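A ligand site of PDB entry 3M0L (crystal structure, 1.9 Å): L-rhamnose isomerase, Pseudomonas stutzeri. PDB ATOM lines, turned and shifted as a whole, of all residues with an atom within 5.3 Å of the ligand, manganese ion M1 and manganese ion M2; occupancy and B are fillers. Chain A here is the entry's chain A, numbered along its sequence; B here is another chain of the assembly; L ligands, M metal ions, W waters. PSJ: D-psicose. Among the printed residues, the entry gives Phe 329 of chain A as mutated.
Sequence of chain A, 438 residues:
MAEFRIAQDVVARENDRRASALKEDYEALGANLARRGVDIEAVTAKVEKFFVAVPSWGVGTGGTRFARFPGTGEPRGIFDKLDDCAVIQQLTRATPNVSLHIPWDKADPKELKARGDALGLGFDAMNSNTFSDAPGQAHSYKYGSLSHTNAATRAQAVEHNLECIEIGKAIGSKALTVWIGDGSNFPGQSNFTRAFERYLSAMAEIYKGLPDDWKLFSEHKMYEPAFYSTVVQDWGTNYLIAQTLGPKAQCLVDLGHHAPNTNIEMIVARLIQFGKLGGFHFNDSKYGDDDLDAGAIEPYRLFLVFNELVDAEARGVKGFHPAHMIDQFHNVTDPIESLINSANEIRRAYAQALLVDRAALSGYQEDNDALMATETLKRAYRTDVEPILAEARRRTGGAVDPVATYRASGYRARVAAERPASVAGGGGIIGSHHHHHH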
ATOM      1  N   TRP A  57     -31.076  27.397 -13.142  1.00  0.00           N
ATOM      2  CA  TRP A  57     -31.602  27.953 -11.907  1.00  0.00           C
ATOM      3  C   TRP A  57     -31.159  29.383 -11.622  1.00  0.00           C
ATOM      4  O   TRP A  57     -31.587  29.997 -10.648  1.00  0.00           O
ATOM      5  CB  TRP A  57     -31.244  27.038 -10.740  1.00  0.00           C
ATOM      6  CG  TRP A  57     -29.770  26.881 -10.493  1.00  0.00           C
ATOM      7  CD1 TRP A  57     -28.980  27.655  -9.690  1.00  0.00           C
ATOM      8  CD2 TRP A  57     -28.909  25.865 -11.042  1.00  0.00           C
ATOM      9  NE1 TRP A  57     -27.682  27.191  -9.710  1.00  0.00           N
ATOM     10  CE2 TRP A  57     -27.620  26.090 -10.528  1.00  0.00           C
ATOM     11  CE3 TRP A  57     -29.120  24.803 -11.927  1.00  0.00           C
ATOM     12  CZ2 TRP A  57     -26.524  25.287 -10.873  1.00  0.00           C
ATOM     13  CZ3 TRP A  57     -28.032  23.988 -12.260  1.00  0.00           C
ATOM     14  CH2 TRP A  57     -26.754  24.245 -11.732  1.00  0.00           C
ATOM     15  N   HIS A 101     -30.954  21.073 -13.949  1.00  0.00           N
ATOM     16  CA  HIS A 101     -31.121  20.547 -12.601  1.00  0.00           C
ATOM     17  C   HIS A 101     -32.407  19.733 -12.581  1.00  0.00           C
ATOM     18  O   HIS A 101     -33.477  20.231 -12.944  1.00  0.00           O
ATOM     19  CB  HIS A 101     -31.198  21.692 -11.596  1.00  0.00           C
ATOM     20  CG  HIS A 101     -30.504  21.406 -10.307  1.00  0.00           C
ATOM     21  ND1 HIS A 101     -30.870  20.379  -9.457  1.00  0.00           N
ATOM     22  CD2 HIS A 101     -29.434  22.004  -9.717  1.00  0.00           C
ATOM     23  CE1 HIS A 101     -30.064  20.355  -8.414  1.00  0.00           C
ATOM     24  NE2 HIS A 101     -29.184  21.325  -8.547  1.00  0.00           N
ATOM     25  N   TRP A 104     -36.120  19.934 -11.122  1.00  0.00           N
ATOM     26  CA  TRP A 104     -36.572  21.267 -11.498  1.00  0.00           C
ATOM     27  C   TRP A 104     -36.839  21.416 -12.998  1.00  0.00           C
ATOM     28  O   TRP A 104     -37.879  21.927 -13.401  1.00  0.00           O
ATOM     29  CB  TRP A 104     -35.557  22.350 -11.077  1.00  0.00           C
ATOM     30  CG  TRP A 104     -35.348  22.496  -9.607  1.00  0.00           C
ATOM     31  CD1 TRP A 104     -36.196  22.088  -8.607  1.00  0.00           C
ATOM     32  CD2 TRP A 104     -34.221  23.099  -8.958  1.00  0.00           C
ATOM     33  NE1 TRP A 104     -35.650  22.400  -7.384  1.00  0.00           N
ATOM     34  CE2 TRP A 104     -34.438  23.019  -7.572  1.00  0.00           C
ATOM     35  CE3 TRP A 104     -33.042  23.696  -9.430  1.00  0.00           C
ATOM     36  CZ2 TRP A 104     -33.524  23.520  -6.634  1.00  0.00           C
ATOM     37  CZ3 TRP A 104     -32.130  24.188  -8.494  1.00  0.00           C
ATOM     38  CH2 TRP A 104     -32.376  24.097  -7.123  1.00  0.00           C
ATOM     39  N   ASN A 127     -27.353  17.946 -13.136  1.00  0.00           N
ATOM     40  CA  ASN A 127     -27.291  18.157 -11.702  1.00  0.00           C
ATOM     41  C   ASN A 127     -28.455  17.412 -11.061  1.00  0.00           C
ATOM     42  O   ASN A 127     -29.607  17.618 -11.443  1.00  0.00           O
ATOM     43  CB  ASN A 127     -27.410  19.648 -11.372  1.00  0.00           C
ATOM     44  CG  ASN A 127     -26.230  20.456 -11.888  1.00  0.00           C
ATOM     45  OD1 ASN A 127     -25.225  20.625 -11.200  1.00  0.00           O
ATOM     46  ND2 ASN A 127     -26.352  20.969 -13.113  1.00  0.00           N
ATOM     47  N   SER A 128     -28.153  16.548 -10.102  1.00  0.00           N
ATOM     48  CA  SER A 128     -29.198  15.794  -9.407  1.00  0.00           C
ATOM     49  C   SER A 128     -29.687  16.564  -8.183  1.00  0.00           C
ATOM     50  O   SER A 128     -29.007  17.457  -7.690  1.00  0.00           O
ATOM     51  CB  SER A 128     -28.663  14.416  -8.975  1.00  0.00           C
ATOM     52  OG  SER A 128     -27.501  14.544  -8.179  1.00  0.00           O
ATOM     53  N   PHE A 131     -31.675  16.824  -2.166  1.00  0.00           N
ATOM     54  CA  PHE A 131     -31.574  17.699  -1.002  1.00  0.00           C
ATOM     55  C   PHE A 131     -32.930  18.363  -0.741  1.00  0.00           C
ATOM     56  O   PHE A 131     -33.048  19.293   0.054  1.00  0.00           O
ATOM     57  CB  PHE A 131     -30.477  18.765  -1.228  1.00  0.00           C
ATOM     58  CG  PHE A 131     -30.622  19.558  -2.499  1.00  0.00           C
ATOM     59  CD1 PHE A 131     -31.565  20.566  -2.601  1.00  0.00           C
ATOM     60  CD2 PHE A 131     -29.808  19.301  -3.589  1.00  0.00           C
ATOM     61  CE1 PHE A 131     -31.697  21.312  -3.770  1.00  0.00           C
ATOM     62  CE2 PHE A 131     -29.924  20.034  -4.768  1.00  0.00           C
ATOM     63  CZ  PHE A 131     -30.874  21.041  -4.856  1.00  0.00           C
ATOM     64  N   TRP A 179     -24.310  17.103  -5.735  1.00  0.00           N
ATOM     65  CA  TRP A 179     -24.160  17.906  -4.534  1.00  0.00           C
ATOM     66  C   TRP A 179     -25.364  17.552  -3.675  1.00  0.00           C
ATOM     67  O   TRP A 179     -26.491  17.594  -4.152  1.00  0.00           O
ATOM     68  CB  TRP A 179     -24.197  19.411  -4.807  1.00  0.00           C
ATOM     69  CG  TRP A 179     -24.228  20.169  -3.498  1.00  0.00           C
ATOM     70  CD1 TRP A 179     -23.182  20.363  -2.639  1.00  0.00           C
ATOM     71  CD2 TRP A 179     -25.378  20.728  -2.857  1.00  0.00           C
ATOM     72  NE1 TRP A 179     -23.618  20.993  -1.502  1.00  0.00           N
ATOM     73  CE2 TRP A 179     -24.956  21.232  -1.605  1.00  0.00           C
ATOM     74  CE3 TRP A 179     -26.737  20.838  -3.205  1.00  0.00           C
ATOM     75  CZ2 TRP A 179     -25.837  21.832  -0.693  1.00  0.00           C
ATOM     76  CZ3 TRP A 179     -27.609  21.449  -2.303  1.00  0.00           C
ATOM     77  CH2 TRP A 179     -27.162  21.940  -1.065  1.00  0.00           C
ATOM     78  N   GLU A 219     -19.385  17.483  -5.451  1.00  0.00           N
ATOM     79  CA  GLU A 219     -19.144  18.854  -5.024  1.00  0.00           C
ATOM     80  C   GLU A 219     -19.154  19.022  -3.511  1.00  0.00           C
ATOM     81  O   GLU A 219     -20.174  18.788  -2.859  1.00  0.00           O
ATOM     82  CB  GLU A 219     -20.195  19.763  -5.673  1.00  0.00           C
ATOM     83  CG  GLU A 219     -20.127  21.230  -5.252  1.00  0.00           C
ATOM     84  CD  GLU A 219     -21.175  22.091  -5.929  1.00  0.00           C
ATOM     85  OE1 GLU A 219     -22.084  21.523  -6.590  1.00  0.00           O
ATOM     86  OE2 GLU A 219     -21.110  23.322  -5.804  1.00  0.00           O
ATOM     87  N   LYS A 221     -18.914  21.039   0.223  1.00  0.00           N
ATOM     88  CA  LYS A 221     -19.446  22.264   0.807  1.00  0.00           C
ATOM     89  C   LYS A 221     -19.299  22.162   2.321  1.00  0.00           C
ATOM     90  O   LYS A 221     -19.715  21.183   2.926  1.00  0.00           O
ATOM     91  CB  LYS A 221     -20.922  22.438   0.444  1.00  0.00           C
ATOM     92  CG  LYS A 221     -21.456  23.826   0.782  1.00  0.00           C
ATOM     93  CD  LYS A 221     -22.933  23.972   0.400  1.00  0.00           C
ATOM     94  CE  LYS A 221     -23.407  25.398   0.605  1.00  0.00           C
ATOM     95  NZ  LYS A 221     -24.871  25.541   0.361  1.00  0.00           N
ATOM     96  N   GLU A 224     -24.382  24.189   5.273  1.00  0.00           N
ATOM     97  CA  GLU A 224     -25.638  24.631   4.661  1.00  0.00           C
ATOM     98  C   GLU A 224     -26.007  23.662   3.541  1.00  0.00           C
ATOM     99  O   GLU A 224     -25.339  23.594   2.510  1.00  0.00           O
ATOM    100  CB  GLU A 224     -25.560  26.053   4.086  1.00  0.00           C
ATOM    101  CG  GLU A 224     -26.939  26.531   3.585  1.00  0.00           C
ATOM    102  CD  GLU A 224     -26.887  27.742   2.675  1.00  0.00           C
ATOM    103  OE1 GLU A 224     -25.903  27.900   1.934  1.00  0.00           O
ATOM    104  OE2 GLU A 224     -27.859  28.541   2.684  1.00  0.00           O
ATOM    105  N   LEU A 252     -15.427  18.814  -8.044  1.00  0.00           N
ATOM    106  CA  LEU A 252     -15.909  20.096  -8.527  1.00  0.00           C
ATOM    107  C   LEU A 252     -15.748  21.102  -7.397  1.00  0.00           C
ATOM    108  O   LEU A 252     -16.136  20.847  -6.260  1.00  0.00           O
ATOM    109  CB  LEU A 252     -17.370  19.978  -8.966  1.00  0.00           C
ATOM    110  CG  LEU A 252     -17.948  21.200  -9.687  1.00  0.00           C
ATOM    111  CD1 LEU A 252     -19.028  20.761 -10.679  1.00  0.00           C
ATOM    112  CD2 LEU A 252     -18.502  22.171  -8.665  1.00  0.00           C
ATOM    113  N   ASP A 254     -16.655  24.753  -5.891  1.00  0.00           N
ATOM    114  CA  ASP A 254     -17.588  25.871  -5.928  1.00  0.00           C
ATOM    115  C   ASP A 254     -16.923  26.919  -5.047  1.00  0.00           C
ATOM    116  O   ASP A 254     -16.747  26.716  -3.853  1.00  0.00           O
ATOM    117  CB  ASP A 254     -18.935  25.479  -5.352  1.00  0.00           C
ATOM    118  CG  ASP A 254     -19.968  26.586  -5.467  1.00  0.00           C
ATOM    119  OD1 ASP A 254     -19.659  27.724  -5.061  1.00  0.00           O
ATOM    120  OD2 ASP A 254     -21.090  26.314  -5.956  1.00  0.00           O
ATOM    121  N   HIS A 257     -17.937  27.701  -1.329  1.00  0.00           N
ATOM    122  CA  HIS A 257     -18.134  26.574  -0.405  1.00  0.00           C
ATOM    123  C   HIS A 257     -16.990  26.284   0.574  1.00  0.00           C
ATOM    124  O   HIS A 257     -16.897  25.179   1.110  1.00  0.00           O
ATOM    125  CB  HIS A 257     -18.424  25.299  -1.196  1.00  0.00           C
ATOM    126  CG  HIS A 257     -19.730  25.302  -1.908  1.00  0.00           C
ATOM    127  ND1 HIS A 257     -20.264  24.175  -2.496  1.00  0.00           N
ATOM    128  CD2 HIS A 257     -20.635  26.285  -2.121  1.00  0.00           C
ATOM    129  CE1 HIS A 257     -21.434  24.463  -3.033  1.00  0.00           C
ATOM    130  NE2 HIS A 257     -21.684  25.737  -2.814  1.00  0.00           N
ATOM    131  N   HIS A 281     -17.535  25.877 -10.189  1.00  0.00           N
ATOM    132  CA  HIS A 281     -18.848  26.483 -10.040  1.00  0.00           C
ATOM    133  C   HIS A 281     -18.446  27.895  -9.636  1.00  0.00           C
ATOM    134  O   HIS A 281     -18.011  28.128  -8.498  1.00  0.00           O
ATOM    135  CB  HIS A 281     -19.666  25.821  -8.932  1.00  0.00           C
ATOM    136  CG  HIS A 281     -20.618  24.770  -9.421  1.00  0.00           C
ATOM    137  ND1 HIS A 281     -21.644  24.276  -8.639  1.00  0.00           N
ATOM    138  CD2 HIS A 281     -20.705  24.128 -10.605  1.00  0.00           C
ATOM    139  CE1 HIS A 281     -22.310  23.363  -9.332  1.00  0.00           C
ATOM    140  NE2 HIS A 281     -21.757  23.254 -10.523  1.00  0.00           N
ATOM    141  N   ASP A 289     -21.892  31.012   1.556  1.00  0.00           N
ATOM    142  CA  ASP A 289     -22.125  30.598   0.176  1.00  0.00           C
ATOM    143  C   ASP A 289     -23.147  31.593  -0.379  1.00  0.00           C
ATOM    144  O   ASP A 289     -24.271  31.232  -0.707  1.00  0.00           O
ATOM    145  CB  ASP A 289     -22.661  29.175   0.139  1.00  0.00           C
ATOM    146  CG  ASP A 289     -22.912  28.680  -1.283  1.00  0.00           C
ATOM    147  OD1 ASP A 289     -22.168  29.104  -2.196  1.00  0.00           O
ATOM    148  OD2 ASP A 289     -23.830  27.858  -1.478  1.00  0.00           O
ATOM    149  N   ASP A 291     -23.393  33.109  -3.161  1.00  0.00           N
ATOM    150  CA  ASP A 291     -23.794  32.939  -4.558  1.00  0.00           C
ATOM    151  C   ASP A 291     -23.991  34.247  -5.313  1.00  0.00           C
ATOM    152  O   ASP A 291     -24.923  34.371  -6.112  1.00  0.00           O
ATOM    153  CB  ASP A 291     -25.054  32.091  -4.648  1.00  0.00           C
ATOM    154  CG  ASP A 291     -24.772  30.624  -4.430  1.00  0.00           C
ATOM    155  OD1 ASP A 291     -23.750  30.155  -4.962  1.00  0.00           O
ATOM    156  OD2 ASP A 291     -25.575  29.943  -3.755  1.00  0.00           O
ATOM    157  N   ASP A 327     -22.553  29.134 -10.968  1.00  0.00           N
ATOM    158  CA  ASP A 327     -23.545  28.662 -10.002  1.00  0.00           C
ATOM    159  C   ASP A 327     -23.847  29.856  -9.111  1.00  0.00           C
ATOM    160  O   ASP A 327     -23.186  30.087  -8.111  1.00  0.00           O
ATOM    161  CB  ASP A 327     -23.023  27.507  -9.149  1.00  0.00           C
ATOM    162  CG  ASP A 327     -24.073  27.011  -8.159  1.00  0.00           C
ATOM    163  OD1 ASP A 327     -25.141  27.656  -8.064  1.00  0.00           O
ATOM    164  OD2 ASP A 327     -23.842  25.997  -7.478  1.00  0.00           O
ATOM    165  N   PHE A 329     -27.154  32.774  -7.698  1.00  0.00           N
ATOM    166  CA  PHE A 329     -28.557  33.075  -7.503  1.00  0.00           C
ATOM    167  C   PHE A 329     -28.646  34.589  -7.532  1.00  0.00           C
ATOM    168  O   PHE A 329     -27.787  35.291  -6.987  1.00  0.00           O
ATOM    169  CB  PHE A 329     -29.072  32.520  -6.170  1.00  0.00           C
ATOM    170  CG  PHE A 329     -29.363  31.047  -6.201  1.00  0.00           C
ATOM    171  CD1 PHE A 329     -28.425  30.122  -5.771  1.00  0.00           C
ATOM    172  CD2 PHE A 329     -30.557  30.572  -6.740  1.00  0.00           C
ATOM    173  CE1 PHE A 329     -28.669  28.746  -5.855  1.00  0.00           C
ATOM    174  CE2 PHE A 329     -30.816  29.203  -6.839  1.00  0.00           C
ATOM    175  CZ  PHE A 329     -29.862  28.293  -6.399  1.00  0.00           C
ATOM    176  N   ARG B  65     -32.822  27.669   2.745  1.00  0.00           N
ATOM    177  CA  ARG B  65     -33.224  28.153   1.435  1.00  0.00           C
ATOM    178  C   ARG B  65     -33.338  26.986   0.449  1.00  0.00           C
ATOM    179  O   ARG B  65     -33.923  27.123  -0.628  1.00  0.00           O
ATOM    180  CB  ARG B  65     -32.237  29.191   0.896  1.00  0.00           C
ATOM    181  CG  ARG B  65     -30.819  28.695   0.755  1.00  0.00           C
ATOM    182  CD  ARG B  65     -29.947  29.640  -0.083  1.00  0.00           C
ATOM    183  NE  ARG B  65     -28.545  29.251   0.016  1.00  0.00           N
ATOM    184  CZ  ARG B  65     -27.632  29.420  -0.929  1.00  0.00           C
ATOM    185  NH1 ARG B  65     -27.942  29.976  -2.094  1.00  0.00           N
ATOM    186  NH2 ARG B  65     -26.388  29.007  -0.702  1.00  0.00           N
ATOM    187  N   PHE B  66     -32.794  25.831   0.826  1.00  0.00           N
ATOM    188  CA  PHE B  66     -32.836  24.637  -0.028  1.00  0.00           C
ATOM    189  C   PHE B  66     -34.063  23.759   0.160  1.00  0.00           C
ATOM    190  O   PHE B  66     -34.534  23.123  -0.793  1.00  0.00           O
ATOM    191  CB  PHE B  66     -31.585  23.794   0.181  1.00  0.00           C
ATOM    192  CG  PHE B  66     -30.343  24.428  -0.336  1.00  0.00           C
ATOM    193  CD1 PHE B  66     -30.107  24.511  -1.706  1.00  0.00           C
ATOM    194  CD2 PHE B  66     -29.415  24.996   0.530  1.00  0.00           C
ATOM    195  CE1 PHE B  66     -28.977  25.147  -2.203  1.00  0.00           C
ATOM    196  CE2 PHE B  66     -28.287  25.628   0.055  1.00  0.00           C
ATOM    197  CZ  PHE B  66     -28.065  25.715  -1.321  1.00  0.00           C
HETATM  198  C1  PSJ L   1     -25.457  24.118  -3.257  1.00  0.00           C
HETATM  199  O1  PSJ L   1     -24.795  24.968  -2.338  1.00  0.00           O
HETATM  200  C2  PSJ L   1     -24.675  24.057  -4.572  1.00  0.00           C
HETATM  201  O2  PSJ L   1     -23.867  24.952  -4.858  1.00  0.00           O
HETATM  202  C3  PSJ L   1     -25.072  23.020  -5.603  1.00  0.00           C
HETATM  203  O3  PSJ L   1     -24.241  23.142  -6.755  1.00  0.00           O
HETATM  204  C4  PSJ L   1     -26.540  23.212  -6.007  1.00  0.00           C
HETATM  205  O4  PSJ L   1     -26.996  22.081  -6.747  1.00  0.00           O
HETATM  206  C5  PSJ L   1     -26.727  24.492  -6.831  1.00  0.00           C
HETATM  207  O5  PSJ L   1     -26.228  25.607  -6.112  1.00  0.00           O
HETATM  208  C6  PSJ L   1     -28.199  24.694  -7.141  1.00  0.00           C
HETATM  209  O6  PSJ L   1     -28.908  24.975  -5.938  1.00  0.00           O
HETATM  210 MN    MN M   1     -22.350  24.762  -6.782  1.00  0.00          MN
HETATM  211 MN    MN M   2     -23.679  26.455  -3.170  1.00  0.00          MN
HETATM  212  O   HOH W   1     -25.228  20.516  -8.323  1.00  0.00           O
HETATM  213  O   HOH W   2     -25.564  27.231  -3.891  1.00  0.00           O
HETATM  214  O   HOH W   3     -22.946  27.960  -4.145  1.00  0.00           O
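The side-chain amino group (NZ) of Lys 221 lies close to an oxygen (O1) of the ligand (2.8 Å). A ring nitrogen (NE2) of His 101 lies within hydrogen-bond range of an oxygen (O4) of the ligand.
OD1 of Asp 327 lies within hydrogen-bond range of NE1 of Trp 57 (3.1 Å). OD2 of Asp 289 lies close to NZ of Lys 221. NH2 of Arg 65 of chain B lies within hydrogen-bond range of O of Asp 289, 3.1 Å away. NZ of Lys 221 lies within salt-bridge range of OE1 of Glu 224, at 3.0 Å. The backbone NH of Phe 329 sits at hydrogen-bond distance from the backbone carbonyl oxygen of Asp 291, 3.2 Å away.
Water W2 bridges OD2 of Asp 291 and O5 of the ligand. Water W3 lies within hydrogen-bond range of OD1 of Asp 291 (2.5 Å) and OD1 of Asp 254 (3.4 Å). Water W1 bridges an oxygen (O4) of the ligand (2.8 Å) and the side-chain amide oxygen of Asn 127 (2.9 Å).
Residues that only touch the ligand: Trp 179, Phe 329, Phe 66 of chain B, Trp 57 and Trp 104. Hydrophobic or aromatic side chains within 4 Å of the ligand: Trp 57, His 101, Trp 104, Trp 179, His 257, His 281, Phe 329 and Phe 66 of chain B. Within 4 Å of the ligand: Trp 57, His 101, Trp 104, Trp 179, Glu 219, Lys 221, Asp 254, His 257, His 281, Asp 289, Asp 327, Phe 329 and Phe 66 of chain B. The nearest printed residue that does not touch the ligand is Phe 131 (4.1 Å).
Manganese ion M1 is bound by ND1 of His 281 (2.0 Å), OD2 of Asp 327 (2.1 Å), OE2 of Glu 219 (2.1 Å), OD2 of Asp 254 (2.2 Å), O2 of the ligand (2.5 Å) and O3 of the ligand (2.5 Å).
Water W3 binds manganese ion M2. O1 of the ligand binds manganese ion M2. NE2 of His 257 is bound to manganese ion M2 (2.1 Å). Manganese ion M2 is bound by water W2 (2.2 Å). OD2 of Asp 289 binds manganese ion M2, at 2.2 Å. Manganese ion M2 is bound by O2 of the ligand, at 2.3 Å.
Lys 221 touches manganese ion M2. Four residues have an atom within 4 Å of manganese ion M2: Lys 221, Asp 254, His 257 and Asp 289. Along chain A the residues within 4 Å of manganese ion M2 span positions 221 to 289. The nearest printed residue that does not touch manganese ion M2 is Asp 291 (4.01 Å).
The nearest printed residue that does not touch manganese ion M1 is Leu 252 (5.0 Å).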
